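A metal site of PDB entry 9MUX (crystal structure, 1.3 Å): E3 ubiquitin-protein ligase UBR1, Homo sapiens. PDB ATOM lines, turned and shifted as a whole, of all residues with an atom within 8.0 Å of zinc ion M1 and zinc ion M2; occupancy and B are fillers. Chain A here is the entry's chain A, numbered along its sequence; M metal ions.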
ATOM      1  N   GLN A   6     -23.909  31.977 -10.796  1.00  0.00           N
ATOM      2  CA  GLN A   6     -25.023  31.069 -10.539  1.00  0.00           C
ATOM      3  C   GLN A   6     -24.810  30.268  -9.261  1.00  0.00           C
ATOM      4  O   GLN A   6     -25.747  30.065  -8.482  1.00  0.00           O
ATOM      5  CB  GLN A   6     -25.203  30.135 -11.738  1.00  0.00           C
ATOM      6  CG  GLN A   6     -23.950  29.297 -12.056  1.00  0.00           C
ATOM      7  CD  GLN A   6     -24.057  28.446 -13.305  1.00  0.00           C
ATOM      8  OE1 GLN A   6     -24.982  28.593 -14.101  1.00  0.00           O
ATOM      9  NE2 GLN A   6     -23.106  27.530 -13.463  1.00  0.00           N
ATOM     10  N   LEU A   7     -23.595  29.805  -9.037  1.00  0.00           N
ATOM     11  CA  LEU A   7     -23.210  29.110  -7.828  1.00  0.00           C
ATOM     12  C   LEU A   7     -22.315  30.035  -7.026  1.00  0.00           C
ATOM     13  O   LEU A   7     -21.873  31.087  -7.508  1.00  0.00           O
ATOM     14  CB  LEU A   7     -22.461  27.814  -8.181  1.00  0.00           C
ATOM     15  CG  LEU A   7     -23.319  26.885  -9.050  1.00  0.00           C
ATOM     16  CD1 LEU A   7     -22.429  25.964  -9.871  1.00  0.00           C
ATOM     17  CD2 LEU A   7     -24.311  26.100  -8.193  1.00  0.00           C
ATOM     18  N   CYS A   8     -22.057  29.647  -5.793  1.00  0.00           N
ATOM     19  CA  CYS A   8     -21.280  30.507  -4.918  1.00  0.00           C
ATOM     20  C   CYS A   8     -19.862  30.733  -5.438  1.00  0.00           C
ATOM     21  O   CYS A   8     -19.496  31.863  -5.802  1.00  0.00           O
ATOM     22  CB  CYS A   8     -21.192  29.918  -3.517  1.00  0.00           C
ATOM     23  SG  CYS A   8     -20.230  31.024  -2.488  1.00  0.00           S
ATOM     24  N   GLY A   9     -19.057  29.680  -5.428  1.00  0.00           N
ATOM     25  CA  GLY A   9     -17.673  29.771  -5.864  1.00  0.00           C
ATOM     26  C   GLY A   9     -16.820  30.790  -5.133  1.00  0.00           C
ATOM     27  O   GLY A   9     -15.837  31.280  -5.709  1.00  0.00           O
ATOM     28  N   ARG A  10     -17.099  31.075  -3.865  1.00  0.00           N
ATOM     29  CA  ARG A  10     -16.267  32.053  -3.162  1.00  0.00           C
ATOM     30  C   ARG A  10     -14.862  31.477  -3.005  1.00  0.00           C
ATOM     31  O   ARG A  10     -14.691  30.340  -2.558  1.00  0.00           O
ATOM     32  CB  ARG A  10     -16.849  32.381  -1.796  1.00  0.00           C
ATOM     33  CG  ARG A  10     -16.119  33.549  -1.125  1.00  0.00           C
ATOM     34  CD  ARG A  10     -16.520  33.773   0.313  1.00  0.00           C
ATOM     35  NE  ARG A  10     -15.893  34.962   0.864  1.00  0.00           N
ATOM     36  CZ  ARG A  10     -16.491  36.149   0.966  1.00  0.00           C
ATOM     37  NH1 ARG A  10     -17.739  36.320   0.574  1.00  0.00           N
ATOM     38  NH2 ARG A  10     -15.815  37.169   1.478  1.00  0.00           N
ATOM     39  N   VAL A  11     -13.850  32.240  -3.402  1.00  0.00           N
ATOM     40  CA  VAL A  11     -12.446  31.866  -3.191  1.00  0.00           C
ATOM     41  C   VAL A  11     -11.980  32.551  -1.919  1.00  0.00           C
ATOM     42  O   VAL A  11     -12.044  33.779  -1.804  1.00  0.00           O
ATOM     43  CB  VAL A  11     -11.560  32.269  -4.382  1.00  0.00           C
ATOM     44  CG1 VAL A  11     -10.092  32.044  -4.049  1.00  0.00           C
ATOM     45  CG2 VAL A  11     -11.941  31.484  -5.611  1.00  0.00           C
ATOM     46  N   PHE A  12     -11.506  31.773  -0.959  1.00  0.00           N
ATOM     47  CA  PHE A  12     -11.144  32.321   0.338  1.00  0.00           C
ATOM     48  C   PHE A  12      -9.831  33.085   0.292  1.00  0.00           C
ATOM     49  O   PHE A  12      -8.898  32.688  -0.408  1.00  0.00           O
ATOM     50  CB  PHE A  12     -11.054  31.204   1.377  1.00  0.00           C
ATOM     51  CG  PHE A  12     -12.355  30.515   1.575  1.00  0.00           C
ATOM     52  CD1 PHE A  12     -13.420  31.183   2.157  1.00  0.00           C
ATOM     53  CD2 PHE A  12     -12.528  29.202   1.159  1.00  0.00           C
ATOM     54  CE1 PHE A  12     -14.644  30.558   2.341  1.00  0.00           C
ATOM     55  CE2 PHE A  12     -13.754  28.564   1.340  1.00  0.00           C
ATOM     56  CZ  PHE A  12     -14.817  29.244   1.925  1.00  0.00           C
ATOM     57  N   VAL A  31     -15.943  22.324   2.235  1.00  0.00           N
ATOM     58  CA  VAL A  31     -16.079  23.520   3.053  1.00  0.00           C
ATOM     59  C   VAL A  31     -17.127  24.447   2.449  1.00  0.00           C
ATOM     60  O   VAL A  31     -17.455  24.365   1.276  1.00  0.00           O
ATOM     61  CB  VAL A  31     -14.731  24.285   3.204  1.00  0.00           C
ATOM     62  CG1 VAL A  31     -13.737  23.491   4.041  1.00  0.00           C
ATOM     63  CG2 VAL A  31     -14.155  24.633   1.815  1.00  0.00           C
ATOM     64  N   LEU A  32     -17.623  25.336   3.295  1.00  0.00           N
ATOM     65  CA  LEU A  32     -18.588  26.341   2.903  1.00  0.00           C
ATOM     66  C   LEU A  32     -18.106  27.701   3.382  1.00  0.00           C
ATOM     67  O   LEU A  32     -17.485  27.812   4.446  1.00  0.00           O
ATOM     68  CB  LEU A  32     -19.925  26.063   3.563  1.00  0.00           C
ATOM     69  CG  LEU A  32     -20.681  24.791   3.104  1.00  0.00           C
ATOM     70  CD1 LEU A  32     -21.903  24.556   4.002  1.00  0.00           C
ATOM     71  CD2 LEU A  32     -21.099  24.859   1.650  1.00  0.00           C
ATOM     72  N   CYS A  33     -18.421  28.729   2.608  1.00  0.00           N
ATOM     73  CA  CYS A  33     -18.238  30.074   3.121  1.00  0.00           C
ATOM     74  C   CYS A  33     -19.283  30.352   4.203  1.00  0.00           C
ATOM     75  O   CYS A  33     -20.234  29.595   4.397  1.00  0.00           O
ATOM     76  CB  CYS A  33     -18.340  31.119   1.997  1.00  0.00           C
ATOM     77  SG  CYS A  33     -20.034  31.340   1.330  1.00  0.00           S
ATOM     78  N   MET A  34     -19.061  31.426   4.960  1.00  0.00           N
ATOM     79  CA  MET A  34     -19.933  31.739   6.074  1.00  0.00           C
ATOM     80  C   MET A  34     -21.374  31.938   5.625  1.00  0.00           C
ATOM     81  O   MET A  34     -22.300  31.440   6.277  1.00  0.00           O
ATOM     82  CB  MET A  34     -19.439  32.983   6.815  1.00  0.00           C
ATOM     83  CG  MET A  34     -20.238  33.288   8.075  1.00  0.00           C
ATOM     84  SD  MET A  34     -19.775  34.850   8.817  1.00  0.00           S
ATOM     85  CE  MET A  34     -20.310  35.980   7.552  1.00  0.00           C
ATOM     86  N   ASP A  35     -21.584  32.667   4.531  1.00  0.00           N
ATOM     87  CA  ASP A  35     -22.949  32.931   4.070  1.00  0.00           C
ATOM     88  C   ASP A  35     -23.662  31.646   3.685  1.00  0.00           C
ATOM     89  O   ASP A  35     -24.806  31.417   4.088  1.00  0.00           O
ATOM     90  CB  ASP A  35     -22.956  33.893   2.887  1.00  0.00           C
ATOM     91  CG  ASP A  35     -22.478  35.271   3.245  1.00  0.00           C
ATOM     92  OD1 ASP A  35     -22.659  35.687   4.398  1.00  0.00           O
ATOM     93  OD2 ASP A  35     -21.938  35.940   2.350  1.00  0.00           O
ATOM     94  N   CYS A  36     -22.995  30.792   2.900  1.00  0.00           N
ATOM     95  CA  CYS A  36     -23.637  29.540   2.511  1.00  0.00           C
ATOM     96  C   CYS A  36     -23.893  28.653   3.729  1.00  0.00           C
ATOM     97  O   CYS A  36     -24.955  28.037   3.830  1.00  0.00           O
ATOM     98  CB  CYS A  36     -22.818  28.815   1.450  1.00  0.00           C
ATOM     99  SG  CYS A  36     -22.794  29.719  -0.126  1.00  0.00           S
ATOM    100  N   PHE A  37     -22.945  28.601   4.657  1.00  0.00           N
ATOM    101  CA  PHE A  37     -23.150  27.822   5.879  1.00  0.00           C
ATOM    102  C   PHE A  37     -24.398  28.311   6.612  1.00  0.00           C
ATOM    103  O   PHE A  37     -25.268  27.515   6.980  1.00  0.00           O
ATOM    104  CB  PHE A  37     -21.917  27.950   6.775  1.00  0.00           C
ATOM    105  CG  PHE A  37     -22.070  27.257   8.085  1.00  0.00           C
ATOM    106  CD1 PHE A  37     -22.021  25.876   8.163  1.00  0.00           C
ATOM    107  CD2 PHE A  37     -22.249  27.982   9.249  1.00  0.00           C
ATOM    108  CE1 PHE A  37     -22.151  25.225   9.389  1.00  0.00           C
ATOM    109  CE2 PHE A  37     -22.377  27.326  10.461  1.00  0.00           C
ATOM    110  CZ  PHE A  37     -22.330  25.959  10.519  1.00  0.00           C
ATOM    111  N   ASP A  39     -26.872  29.948   5.559  1.00  0.00           N
ATOM    112  CA  ASP A  39     -28.078  29.808   4.749  1.00  0.00           C
ATOM    113  C   ASP A  39     -28.395  28.365   4.438  1.00  0.00           C
ATOM    114  O   ASP A  39     -29.242  28.080   3.568  1.00  0.00           O
ATOM    115  CB  ASP A  39     -27.932  30.603   3.449  1.00  0.00           C
ATOM    116  CG  ASP A  39     -28.117  32.084   3.643  1.00  0.00           C
ATOM    117  OD1 ASP A  39     -28.798  32.490   4.612  1.00  0.00           O
ATOM    118  OD2 ASP A  39     -27.566  32.869   2.832  1.00  0.00           O
ATOM    119  N   SER A  40     -27.743  27.430   5.114  1.00  0.00           N
ATOM    120  CA  SER A  40     -27.881  26.009   4.825  1.00  0.00           C
ATOM    121  C   SER A  40     -28.351  25.270   6.078  1.00  0.00           C
ATOM    122  O   SER A  40     -28.272  25.768   7.197  1.00  0.00           O
ATOM    123  CB  SER A  40     -26.552  25.397   4.363  1.00  0.00           C
ATOM    124  OG  SER A  40     -25.701  25.150   5.473  1.00  0.00           O
ATOM    125  N   PHE A  57     -12.013  27.021  -1.963  1.00  0.00           N
ATOM    126  CA  PHE A  57     -13.229  27.619  -2.468  1.00  0.00           C
ATOM    127  C   PHE A  57     -14.435  26.941  -1.844  1.00  0.00           C
ATOM    128  O   PHE A  57     -14.365  25.793  -1.399  1.00  0.00           O
ATOM    129  CB  PHE A  57     -13.279  27.582  -4.001  1.00  0.00           C
ATOM    130  CG  PHE A  57     -13.245  26.197  -4.594  1.00  0.00           C
ATOM    131  CD1 PHE A  57     -12.039  25.590  -4.886  1.00  0.00           C
ATOM    132  CD2 PHE A  57     -14.424  25.520  -4.884  1.00  0.00           C
ATOM    133  CE1 PHE A  57     -12.012  24.303  -5.451  1.00  0.00           C
ATOM    134  CE2 PHE A  57     -14.393  24.259  -5.442  1.00  0.00           C
ATOM    135  CZ  PHE A  57     -13.184  23.666  -5.731  1.00  0.00           C
ATOM    136  N   CYS A  58     -15.538  27.675  -1.793  1.00  0.00           N
ATOM    137  CA  CYS A  58     -16.782  27.184  -1.233  1.00  0.00           C
ATOM    138  C   CYS A  58     -17.377  26.063  -2.089  1.00  0.00           C
ATOM    139  O   CYS A  58     -17.450  26.165  -3.316  1.00  0.00           O
ATOM    140  CB  CYS A  58     -17.771  28.345  -1.135  1.00  0.00           C
ATOM    141  SG  CYS A  58     -19.371  27.874  -0.464  1.00  0.00           S
ATOM    142  N   ASP A  59     -17.840  25.002  -1.419  1.00  0.00           N
ATOM    143  CA  ASP A  59     -18.420  23.832  -2.073  1.00  0.00           C
ATOM    144  C   ASP A  59     -19.933  23.829  -2.073  1.00  0.00           C
ATOM    145  O   ASP A  59     -20.538  22.774  -2.308  1.00  0.00           O
ATOM    146  CB  ASP A  59     -17.911  22.563  -1.413  1.00  0.00           C
ATOM    147  CG  ASP A  59     -16.433  22.374  -1.614  1.00  0.00           C
ATOM    148  OD1 ASP A  59     -15.978  22.442  -2.789  1.00  0.00           O
ATOM    149  OD2 ASP A  59     -15.686  22.214  -0.623  1.00  0.00           O
ATOM    150  N   CYS A  60     -20.565  24.970  -1.834  1.00  0.00           N
ATOM    151  CA  CYS A  60     -22.007  25.030  -1.955  1.00  0.00           C
ATOM    152  C   CYS A  60     -22.425  24.552  -3.340  1.00  0.00           C
ATOM    153  O   CYS A  60     -21.870  24.998  -4.355  1.00  0.00           O
ATOM    154  CB  CYS A  60     -22.463  26.466  -1.740  1.00  0.00           C
ATOM    155  SG  CYS A  60     -24.285  26.626  -1.897  1.00  0.00           S
ATOM    156  N   GLY A  61     -23.357  23.608  -3.375  1.00  0.00           N
ATOM    157  CA  GLY A  61     -23.914  23.150  -4.629  1.00  0.00           C
ATOM    158  C   GLY A  61     -23.339  21.860  -5.164  1.00  0.00           C
ATOM    159  O   GLY A  61     -23.858  21.340  -6.153  1.00  0.00           O
ATOM    160  N   PRO A  70     -26.825  19.811  -0.135  1.00  0.00           N
ATOM    161  CA  PRO A  70     -25.620  20.385  -0.763  1.00  0.00           C
ATOM    162  C   PRO A  70     -25.726  21.859  -1.097  1.00  0.00           C
ATOM    163  O   PRO A  70     -24.672  22.493  -1.259  1.00  0.00           O
ATOM    164  CB  PRO A  70     -25.460  19.552  -2.039  1.00  0.00           C
ATOM    165  CG  PRO A  70     -26.845  19.095  -2.347  1.00  0.00           C
ATOM    166  CD  PRO A  70     -27.504  18.849  -1.032  1.00  0.00           C
ATOM    167  N   PHE A  71     -26.919  22.426  -1.222  1.00  0.00           N
ATOM    168  CA  PHE A  71     -27.088  23.840  -1.541  1.00  0.00           C
ATOM    169  C   PHE A  71     -27.594  24.604  -0.329  1.00  0.00           C
ATOM    170  O   PHE A  71     -28.488  24.129   0.383  1.00  0.00           O
ATOM    171  CB  PHE A  71     -28.149  24.043  -2.649  1.00  0.00           C
ATOM    172  CG  PHE A  71     -27.694  23.677  -4.036  1.00  0.00           C
ATOM    173  CD1 PHE A  71     -27.069  24.611  -4.844  1.00  0.00           C
ATOM    174  CD2 PHE A  71     -27.970  22.424  -4.555  1.00  0.00           C
ATOM    175  CE1 PHE A  71     -26.698  24.288  -6.141  1.00  0.00           C
ATOM    176  CE2 PHE A  71     -27.580  22.087  -5.843  1.00  0.00           C
ATOM    177  CZ  PHE A  71     -26.949  23.022  -6.627  1.00  0.00           C
ATOM    178  N   CYS A  72     -27.085  25.808  -0.119  1.00  0.00           N
ATOM    179  CA  CYS A  72     -27.767  26.747   0.748  1.00  0.00           C
ATOM    180  C   CYS A  72     -29.028  27.263   0.048  1.00  0.00           C
ATOM    181  O   CYS A  72     -29.224  27.089  -1.150  1.00  0.00           O
ATOM    182  CB  CYS A  72     -26.824  27.902   1.103  1.00  0.00           C
ATOM    183  SG  CYS A  72     -26.622  29.168  -0.192  1.00  0.00           S
ATOM    184  N   VAL A  73     -29.876  27.957   0.803  1.00  0.00           N
ATOM    185  CA  VAL A  73     -31.164  28.324   0.231  1.00  0.00           C
ATOM    186  C   VAL A  73     -31.005  29.303  -0.931  1.00  0.00           C
ATOM    187  O   VAL A  73     -31.767  29.248  -1.913  1.00  0.00           O
ATOM    188  CB  VAL A  73     -32.133  28.832   1.320  1.00  0.00           C
ATOM    189  CG1 VAL A  73     -31.679  30.165   1.894  1.00  0.00           C
ATOM    190  CG2 VAL A  73     -33.549  28.969   0.753  1.00  0.00           C
ATOM    191  N   ASN A  74     -30.013  30.195  -0.850  1.00  0.00           N
ATOM    192  CA  ASN A  74     -29.798  31.198  -1.887  1.00  0.00           C
ATOM    193  C   ASN A  74     -29.431  30.535  -3.215  1.00  0.00           C
ATOM    194  O   ASN A  74     -29.929  30.941  -4.267  1.00  0.00           O
ATOM    195  CB  ASN A  74     -28.623  32.089  -1.479  1.00  0.00           C
ATOM    196  CG  ASN A  74     -29.006  33.204  -0.526  1.00  0.00           C
ATOM    197  OD1 ASN A  74     -28.175  34.075  -0.229  1.00  0.00           O
ATOM    198  ND2 ASN A  74     -30.233  33.188  -0.030  1.00  0.00           N
ATOM    199  N   HIS A  75     -28.553  29.546  -3.188  1.00  0.00           N
ATOM    200  CA  HIS A  75     -28.016  28.949  -4.404  1.00  0.00           C
ATOM    201  C   HIS A  75     -28.819  27.756  -4.908  1.00  0.00           C
ATOM    202  O   HIS A  75     -28.633  27.344  -6.053  1.00  0.00           O
ATOM    203  CB  HIS A  75     -26.543  28.576  -4.218  1.00  0.00           C
ATOM    204  CG  HIS A  75     -25.673  29.774  -4.060  1.00  0.00           C
ATOM    205  ND1 HIS A  75     -24.929  30.030  -2.929  1.00  0.00           N
ATOM    206  CD2 HIS A  75     -25.487  30.843  -4.882  1.00  0.00           C
ATOM    207  CE1 HIS A  75     -24.306  31.188  -3.066  1.00  0.00           C
ATOM    208  NE2 HIS A  75     -24.622  31.706  -4.240  1.00  0.00           N
ATOM    209  N   GLU A  76     -29.696  27.224  -4.074  1.00  0.00           N
ATOM    210  CA  GLU A  76     -30.481  26.076  -4.452  1.00  0.00           C
ATOM    211  C   GLU A  76     -31.288  26.383  -5.702  1.00  0.00           C
ATOM    212  O   GLU A  76     -31.993  27.393  -5.730  1.00  0.00           O
ATOM    213  CB  GLU A  76     -31.440  25.820  -3.287  1.00  0.00           C
ATOM    214  CG  GLU A  76     -32.173  24.508  -3.333  1.00  0.00           C
ATOM    215  CD  GLU A  76     -32.650  24.135  -1.946  1.00  0.00           C
ATOM    216  OE1 GLU A  76     -33.410  24.934  -1.338  1.00  0.00           O
ATOM    217  OE2 GLU A  76     -32.210  23.079  -1.456  1.00  0.00           O
HETATM  218 ZN    ZN M   1     -20.450  29.932  -0.495  1.00  0.00          ZN
HETATM  219 ZN    ZN M   2     -24.637  28.815  -1.290  1.00  0.00          ZN
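Of the 28 residues printed, 4 come within 4 Å of zinc ion M1.
Zinc ion M2 is bound by a ring nitrogen (ND1) of His 75 (2.1 Å), the side-chain sulfur of Cys 72 (2.3 Å), the side-chain sulfur of Cys 60 (2.3 Å) and the side-chain sulfur of Cys 36 (2.4 Å). Zinc ion M2 has four donor atoms within binding distance.
Zinc ion M1 is bound by the side-chain sulfur (SG) of Cys 8 (2.3 Å). SG of Cys 58 binds zinc ion M1 (2.3 Å). SG of Cys 33 binds zinc ion M1, at 2.3 Å. Zinc ion M1 is bound by SG of Cys 36, at 2.4 Å. Zinc ion M1 has four donor atoms within binding distance.
Four residues have an atom within 4 Å of zinc ion M2: Cys 36, Cys 60, Cys 72 and His 75.
N of Cys 60 lies close to SG of Cys 58 (3.4 Å). The side-chain hydroxyl (OG) of Ser 40 lies close to the backbone carbonyl oxygen (O) of Cys 36 (3.4 Å). The backbone NH (N) of Arg 10 sits close to the side-chain sulfur (SG) of Cys 8 (3.4 Å). O of Arg 10 is in hydrogen-bond range of N of Cys 58, 2.9 Å away. The side-chain sulfur (SG) of Cys 72 sits close to the backbone NH (N) of Asn 74, 3.6 Å away. The side-chain sulfur (SG) of Cys 33 lies close to the backbone NH (N) of Asp 35, 3.8 Å away.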
